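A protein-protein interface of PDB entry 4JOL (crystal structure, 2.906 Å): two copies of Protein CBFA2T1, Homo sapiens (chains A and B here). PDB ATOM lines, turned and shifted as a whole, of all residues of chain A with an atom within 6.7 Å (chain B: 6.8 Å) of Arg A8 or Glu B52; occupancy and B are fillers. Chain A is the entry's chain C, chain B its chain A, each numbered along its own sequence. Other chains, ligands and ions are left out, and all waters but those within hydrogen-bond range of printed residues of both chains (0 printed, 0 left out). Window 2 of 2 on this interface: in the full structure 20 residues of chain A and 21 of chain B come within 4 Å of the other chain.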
ATOM      1  N   ILE A   5       0.971   4.222   3.702  1.00  0.00           N
ATOM      2  CA  ILE A   5       1.263   5.640   3.903  1.00  0.00           C
ATOM      3  C   ILE A   5       2.575   6.052   3.240  1.00  0.00           C
ATOM      4  O   ILE A   5       3.648   5.903   3.814  1.00  0.00           O
ATOM      5  CB  ILE A   5       1.354   6.005   5.407  1.00  0.00           C
ATOM      6  CG1 ILE A   5      -0.033   6.178   6.023  1.00  0.00           C
ATOM      7  CG2 ILE A   5       2.139   7.298   5.603  1.00  0.00           C
ATOM      8  CD1 ILE A   5       0.011   6.727   7.442  1.00  0.00           C
ATOM      9  N   ASP A   6       2.483   6.557   2.022  1.00  0.00           N
ATOM     10  CA  ASP A   6       3.628   7.171   1.383  1.00  0.00           C
ATOM     11  C   ASP A   6       3.241   8.611   1.083  1.00  0.00           C
ATOM     12  O   ASP A   6       2.357   8.861   0.268  1.00  0.00           O
ATOM     13  CB  ASP A   6       4.009   6.432   0.095  1.00  0.00           C
ATOM     14  CG  ASP A   6       5.192   7.085  -0.629  1.00  0.00           C
ATOM     15  OD1 ASP A   6       6.010   7.756   0.042  1.00  0.00           O
ATOM     16  OD2 ASP A   6       5.306   6.936  -1.869  1.00  0.00           O
ATOM     17  N   HIS A   7       3.889   9.550   1.766  1.00  0.00           N
ATOM     18  CA  HIS A   7       3.630  10.975   1.572  1.00  0.00           C
ATOM     19  C   HIS A   7       4.164  11.510   0.236  1.00  0.00           C
ATOM     20  O   HIS A   7       3.928  12.679  -0.099  1.00  0.00           O
ATOM     21  CB  HIS A   7       4.204  11.811   2.724  1.00  0.00           C
ATOM     22  CG  HIS A   7       3.537  11.576   4.043  1.00  0.00           C
ATOM     23  ND1 HIS A   7       2.725  10.492   4.284  1.00  0.00           N
ATOM     24  CD2 HIS A   7       3.570  12.287   5.197  1.00  0.00           C
ATOM     25  CE1 HIS A   7       2.279  10.546   5.528  1.00  0.00           C
ATOM     26  NE2 HIS A   7       2.778  11.624   6.103  1.00  0.00           N
ATOM     27  N   ARG A   8       4.850  10.673  -0.545  1.00  0.00           N
ATOM     28  CA  ARG A   8       5.333  11.153  -1.826  1.00  0.00           C
ATOM     29  C   ARG A   8       4.142  10.928  -2.724  1.00  0.00           C
ATOM     30  O   ARG A   8       3.865   9.818  -3.162  1.00  0.00           O
ATOM     31  CB  ARG A   8       6.466  10.274  -2.353  1.00  0.00           C
ATOM     32  CG  ARG A   8       7.890  10.600  -1.933  1.00  0.00           C
ATOM     33  CD  ARG A   8       8.875  10.141  -3.032  1.00  0.00           C
ATOM     34  NE  ARG A   8       8.599  10.798  -4.319  1.00  0.00           N
ATOM     35  CZ  ARG A   8       9.308  10.635  -5.441  1.00  0.00           C
ATOM     36  NH1 ARG A   8      10.367   9.823  -5.467  1.00  0.00           N
ATOM     37  NH2 ARG A   8       8.949  11.292  -6.542  1.00  0.00           N
ATOM     38  N   LEU A   9       3.448  12.019  -3.001  1.00  0.00           N
ATOM     39  CA  LEU A   9       2.323  12.050  -3.917  1.00  0.00           C
ATOM     40  C   LEU A   9       2.873  12.020  -5.318  1.00  0.00           C
ATOM     41  O   LEU A   9       4.063  12.202  -5.534  1.00  0.00           O
ATOM     42  CB  LEU A   9       1.455  13.293  -3.700  1.00  0.00           C
ATOM     43  CG  LEU A   9       0.214  13.182  -2.803  1.00  0.00           C
ATOM     44  CD1 LEU A   9       0.376  12.202  -1.642  1.00  0.00           C
ATOM     45  CD2 LEU A   9      -0.185  14.556  -2.299  1.00  0.00           C
ATOM     46  N   THR A  10       2.004  11.751  -6.269  1.00  0.00           N
ATOM     47  CA  THR A  10       2.403  11.668  -7.656  1.00  0.00           C
ATOM     48  C   THR A  10       1.770  12.856  -8.340  1.00  0.00           C
ATOM     49  O   THR A  10       0.801  13.432  -7.832  1.00  0.00           O
ATOM     50  CB  THR A  10       1.907  10.350  -8.311  1.00  0.00           C
ATOM     51  OG1 THR A  10       0.524  10.471  -8.664  1.00  0.00           O
ATOM     52  CG2 THR A  10       2.072   9.201  -7.353  1.00  0.00           C
ATOM     53  N   GLU A  13      -1.842  12.655  -8.498  1.00  0.00           N
ATOM     54  CA  GLU A  13      -2.410  12.812  -7.165  1.00  0.00           C
ATOM     55  C   GLU A  13      -2.312  14.272  -6.724  1.00  0.00           C
ATOM     56  O   GLU A  13      -3.273  14.822  -6.181  1.00  0.00           O
ATOM     57  CB  GLU A  13      -1.716  11.905  -6.147  1.00  0.00           C
ATOM     58  CG  GLU A  13      -1.443  10.502  -6.639  1.00  0.00           C
ATOM     59  CD  GLU A  13      -0.838   9.614  -5.571  1.00  0.00           C
ATOM     60  OE1 GLU A  13       0.363   9.779  -5.269  1.00  0.00           O
ATOM     61  OE2 GLU A  13      -1.562   8.743  -5.043  1.00  0.00           O
ATOM     62  N   TRP A  14      -1.159  14.903  -6.950  1.00  0.00           N
ATOM     63  CA  TRP A  14      -0.993  16.297  -6.535  1.00  0.00           C
ATOM     64  C   TRP A  14      -2.081  17.159  -7.166  1.00  0.00           C
ATOM     65  O   TRP A  14      -2.768  17.922  -6.476  1.00  0.00           O
ATOM     66  CB  TRP A  14       0.403  16.861  -6.867  1.00  0.00           C
ATOM     67  CG  TRP A  14       1.413  16.794  -5.725  1.00  0.00           C
ATOM     68  CD1 TRP A  14       2.539  16.021  -5.679  1.00  0.00           C
ATOM     69  CD2 TRP A  14       1.382  17.526  -4.482  1.00  0.00           C
ATOM     70  NE1 TRP A  14       3.200  16.214  -4.489  1.00  0.00           N
ATOM     71  CE2 TRP A  14       2.515  17.136  -3.740  1.00  0.00           C
ATOM     72  CE3 TRP A  14       0.512  18.466  -3.930  1.00  0.00           C
ATOM     73  CZ2 TRP A  14       2.798  17.655  -2.471  1.00  0.00           C
ATOM     74  CZ3 TRP A  14       0.798  18.975  -2.669  1.00  0.00           C
ATOM     75  CH2 TRP A  14       1.926  18.564  -1.955  1.00  0.00           C
ATOM     76  N   ARG B  44       2.582  17.842   5.053  1.00  0.00           N
ATOM     77  CA  ARG B  44       3.415  16.665   5.216  1.00  0.00           C
ATOM     78  C   ARG B  44       3.824  16.074   3.853  1.00  0.00           C
ATOM     79  O   ARG B  44       4.921  15.542   3.704  1.00  0.00           O
ATOM     80  CB  ARG B  44       2.708  15.635   6.108  1.00  0.00           C
ATOM     81  CG  ARG B  44       3.207  15.623   7.562  1.00  0.00           C
ATOM     82  CD  ARG B  44       2.101  15.335   8.579  1.00  0.00           C
ATOM     83  NE  ARG B  44       1.506  14.013   8.398  1.00  0.00           N
ATOM     84  CZ  ARG B  44       0.241  13.715   8.686  1.00  0.00           C
ATOM     85  NH1 ARG B  44      -0.565  14.657   9.167  1.00  0.00           N
ATOM     86  NH2 ARG B  44      -0.217  12.480   8.484  1.00  0.00           N
ATOM     87  N   CYS B  45       2.960  16.187   2.852  1.00  0.00           N
ATOM     88  CA  CYS B  45       3.315  15.738   1.511  1.00  0.00           C
ATOM     89  C   CYS B  45       4.347  16.642   0.851  1.00  0.00           C
ATOM     90  O   CYS B  45       5.253  16.168   0.169  1.00  0.00           O
ATOM     91  CB  CYS B  45       2.079  15.651   0.624  1.00  0.00           C
ATOM     92  SG  CYS B  45       1.010  14.305   1.058  1.00  0.00           S
ATOM     93  N   GLU B  47       6.486  18.595   2.531  1.00  0.00           N
ATOM     94  CA  GLU B  47       7.719  18.389   3.262  1.00  0.00           C
ATOM     95  C   GLU B  47       8.380  17.047   2.899  1.00  0.00           C
ATOM     96  O   GLU B  47       9.604  16.943   2.815  1.00  0.00           O
ATOM     97  CB  GLU B  47       7.470  18.544   4.770  1.00  0.00           C
ATOM     98  CG  GLU B  47       6.856  19.898   5.133  1.00  0.00           C
ATOM     99  CD  GLU B  47       6.633  20.102   6.630  1.00  0.00           C
ATOM    100  OE1 GLU B  47       6.444  21.269   7.041  1.00  0.00           O
ATOM    101  OE2 GLU B  47       6.638  19.111   7.392  1.00  0.00           O
ATOM    102  N   ALA B  48       7.577  16.019   2.663  1.00  0.00           N
ATOM    103  CA  ALA B  48       8.137  14.729   2.289  1.00  0.00           C
ATOM    104  C   ALA B  48       8.871  14.815   0.940  1.00  0.00           C
ATOM    105  O   ALA B  48       9.951  14.238   0.767  1.00  0.00           O
ATOM    106  CB  ALA B  48       7.056  13.677   2.253  1.00  0.00           C
ATOM    107  N   ASP B  49       8.289  15.534  -0.011  1.00  0.00           N
ATOM    108  CA  ASP B  49       8.958  15.772  -1.279  1.00  0.00           C
ATOM    109  C   ASP B  49      10.322  16.438  -1.089  1.00  0.00           C
ATOM    110  O   ASP B  49      11.248  16.245  -1.887  1.00  0.00           O
ATOM    111  CB  ASP B  49       8.087  16.636  -2.176  1.00  0.00           C
ATOM    112  CG  ASP B  49       7.358  15.829  -3.230  1.00  0.00           C
ATOM    113  OD1 ASP B  49       6.449  15.029  -2.859  1.00  0.00           O
ATOM    114  OD2 ASP B  49       7.706  16.014  -4.428  1.00  0.00           O
ATOM    115  N   ARG B  50      10.449  17.223  -0.027  1.00  0.00           N
ATOM    116  CA  ARG B  50      11.688  17.936   0.203  1.00  0.00           C
ATOM    117  C   ARG B  50      12.753  17.006   0.785  1.00  0.00           C
ATOM    118  O   ARG B  50      13.936  17.090   0.423  1.00  0.00           O
ATOM    119  CB  ARG B  50      11.460  19.125   1.126  1.00  0.00           C
ATOM    120  CG  ARG B  50      12.552  20.170   1.048  1.00  0.00           C
ATOM    121  CD  ARG B  50      12.302  21.101  -0.125  1.00  0.00           C
ATOM    122  NE  ARG B  50      12.281  22.486   0.332  1.00  0.00           N
ATOM    123  CZ  ARG B  50      11.968  23.527  -0.426  1.00  0.00           C
ATOM    124  NH1 ARG B  50      11.644  23.359  -1.704  1.00  0.00           N
ATOM    125  NH2 ARG B  50      11.982  24.736   0.099  1.00  0.00           N
ATOM    126  N   GLU B  51      12.334  16.125   1.691  1.00  0.00           N
ATOM    127  CA  GLU B  51      13.255  15.158   2.260  1.00  0.00           C
ATOM    128  C   GLU B  51      13.810  14.269   1.130  1.00  0.00           C
ATOM    129  O   GLU B  51      14.955  13.801   1.179  1.00  0.00           O
ATOM    130  CB  GLU B  51      12.561  14.336   3.354  1.00  0.00           C
ATOM    131  CG  GLU B  51      13.465  13.982   4.542  1.00  0.00           C
ATOM    132  CD  GLU B  51      14.035  15.215   5.251  1.00  0.00           C
ATOM    133  OE1 GLU B  51      15.268  15.451   5.179  1.00  0.00           O
ATOM    134  OE2 GLU B  51      13.248  15.947   5.888  1.00  0.00           O
ATOM    135  N   GLU B  52      12.996  14.084   0.096  1.00  0.00           N
ATOM    136  CA  GLU B  52      13.344  13.224  -1.014  1.00  0.00           C
ATOM    137  C   GLU B  52      14.369  13.931  -1.878  1.00  0.00           C
ATOM    138  O   GLU B  52      15.387  13.326  -2.286  1.00  0.00           O
ATOM    139  CB  GLU B  52      12.079  12.840  -1.801  1.00  0.00           C
ATOM    140  CG  GLU B  52      12.120  11.462  -2.451  1.00  0.00           C
ATOM    141  CD  GLU B  52      12.718  10.334  -1.552  1.00  0.00           C
ATOM    142  OE1 GLU B  52      12.584  10.353  -0.299  1.00  0.00           O
ATOM    143  OE2 GLU B  52      13.315   9.393  -2.124  1.00  0.00           O
ATOM    144  N   LEU B  53      14.127  15.221  -2.127  1.00  0.00           N
ATOM    145  CA  LEU B  53      15.130  16.046  -2.813  1.00  0.00           C
ATOM    146  C   LEU B  53      16.473  16.051  -2.091  1.00  0.00           C
ATOM    147  O   LEU B  53      17.511  15.917  -2.730  1.00  0.00           O
ATOM    148  CB  LEU B  53      14.644  17.470  -3.024  1.00  0.00           C
ATOM    149  CG  LEU B  53      15.648  18.437  -3.644  1.00  0.00           C
ATOM    150  CD1 LEU B  53      16.187  17.875  -4.918  1.00  0.00           C
ATOM    151  CD2 LEU B  53      15.000  19.777  -3.912  1.00  0.00           C
ATOM    152  N   ASN B  54      16.464  16.175  -0.766  1.00  0.00           N
ATOM    153  CA  ASN B  54      17.728  16.175  -0.028  1.00  0.00           C
ATOM    154  C   ASN B  54      18.429  14.866  -0.252  1.00  0.00           C
ATOM    155  O   ASN B  54      19.657  14.839  -0.460  1.00  0.00           O
ATOM    156  CB  ASN B  54      17.554  16.425   1.479  1.00  0.00           C
ATOM    157  CG  ASN B  54      16.863  17.758   1.796  1.00  0.00           C
ATOM    158  OD1 ASN B  54      16.881  18.706   1.000  1.00  0.00           O
ATOM    159  ND2 ASN B  54      16.248  17.828   2.976  1.00  0.00           N
ATOM    160  N   TYR B  55      17.647  13.782  -0.223  1.00  0.00           N
ATOM    161  CA  TYR B  55      18.199  12.449  -0.449  1.00  0.00           C
ATOM    162  C   TYR B  55      18.941  12.388  -1.769  1.00  0.00           C
ATOM    163  O   TYR B  55      20.072  11.925  -1.826  1.00  0.00           O
ATOM    164  CB  TYR B  55      17.130  11.355  -0.403  1.00  0.00           C
ATOM    165  CG  TYR B  55      17.714  10.002  -0.756  1.00  0.00           C
ATOM    166  CD1 TYR B  55      18.566   9.346   0.122  1.00  0.00           C
ATOM    167  CD2 TYR B  55      17.452   9.406  -1.985  1.00  0.00           C
ATOM    168  CE1 TYR B  55      19.122   8.136  -0.201  1.00  0.00           C
ATOM    169  CE2 TYR B  55      18.005   8.189  -2.316  1.00  0.00           C
ATOM    170  CZ  TYR B  55      18.838   7.562  -1.419  1.00  0.00           C
ATOM    171  OH  TYR B  55      19.392   6.347  -1.735  1.00  0.00           O
ATOM    172  N   TRP B  56      18.303  12.863  -2.829  1.00  0.00           N
ATOM    173  CA  TRP B  56      18.945  12.849  -4.135  1.00  0.00           C
ATOM    174  C   TRP B  56      20.184  13.734  -4.270  1.00  0.00           C
ATOM    175  O   TRP B  56      21.175  13.288  -4.841  1.00  0.00           O
ATOM    176  CB  TRP B  56      17.931  13.129  -5.241  1.00  0.00           C
ATOM    177  CG  TRP B  56      17.097  11.944  -5.465  1.00  0.00           C
ATOM    178  CD1 TRP B  56      15.810  11.757  -5.069  1.00  0.00           C
ATOM    179  CD2 TRP B  56      17.515  10.729  -6.068  1.00  0.00           C
ATOM    180  NE1 TRP B  56      15.388  10.500  -5.410  1.00  0.00           N
ATOM    181  CE2 TRP B  56      16.418   9.845  -6.028  1.00  0.00           C
ATOM    182  CE3 TRP B  56      18.707  10.302  -6.653  1.00  0.00           C
ATOM    183  CZ2 TRP B  56      16.473   8.559  -6.556  1.00  0.00           C
ATOM    184  CZ3 TRP B  56      18.769   9.022  -7.170  1.00  0.00           C
ATOM    185  CH2 TRP B  56      17.656   8.164  -7.120  1.00  0.00           C
ATOM    186  N   ILE B  57      20.124  14.974  -3.759  1.00  0.00           N
ATOM    187  CA  ILE B  57      21.275  15.884  -3.746  1.00  0.00           C
ATOM    188  C   ILE B  57      22.431  15.168  -3.071  1.00  0.00           C
ATOM    189  O   ILE B  57      23.554  15.089  -3.576  1.00  0.00           O
ATOM    190  CB  ILE B  57      21.005  17.131  -2.880  1.00  0.00           C
ATOM    191  CG1 ILE B  57      19.836  17.958  -3.402  1.00  0.00           C
ATOM    192  CG2 ILE B  57      22.221  18.015  -2.855  1.00  0.00           C
ATOM    193  CD1 ILE B  57      20.127  18.563  -4.706  1.00  0.00           C
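Printed residues of chain A that touch a printed residue of chain B: His A7, Arg A8, Leu A9 and Trp A14. Hydrophobic or aromatic side chains of chain A within 4 Å of the printed part of chain B: His A7, Leu A9 and Trp A14. Printed residues of chain B that touch a printed residue of chain A: Arg B44, Cys B45, Ala B48, Asp B49 and Glu B52. Hydrophobic or aromatic side chains of chain B that line the printed part of chain A: Ala B48. Among the printed residues, 7 pairs touch across the chains.
No position is printed for both chains. Of the 7 pairs that touch across the chains among the printed residues, none has its exchanged pair printed and touching as well.
The side-chain sulfur (SG) of Cys B45 sits close to the backbone carbonyl oxygen (O) of His A7.
Of chain B, only Glu B52 (3.6 Å) comes within 4 Å of Arg A8. Of the printed residues of chain B, Leu A9 touches Cys B45 (3.5 Å). Of the printed residues of chain B, Trp A14 touches Cys B45 and Asp B49. Of the printed residues of chain A, Arg B44 touches His A7 (3.5 Å). Of the printed residues of chain A, Cys B45 touches His A7, Leu A9 and Trp A14. Printed residues of chain A within 4 Å of Glu B52: Arg A8. The nearest residue of chain B that does not touch Arg A8 is Asp B49 (4.2 Å). The nearest printed residue of chain A that does not touch Glu B52 is Asp A6 (7.1 Å). The nearest printed residue of chain A that does not touch Asp B49 is Arg A8 (4.2 Å).
N of Arg A8 lies close to OD1 of Asp A6.
Among the printed residues, merely in contact across the chains: His A7 with Ala B48, Leu A9 with Cys B45, His A7 with Arg B44, Arg A8 with Glu B52, Trp A14 with Cys B45 and Trp A14 with Asp B49.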
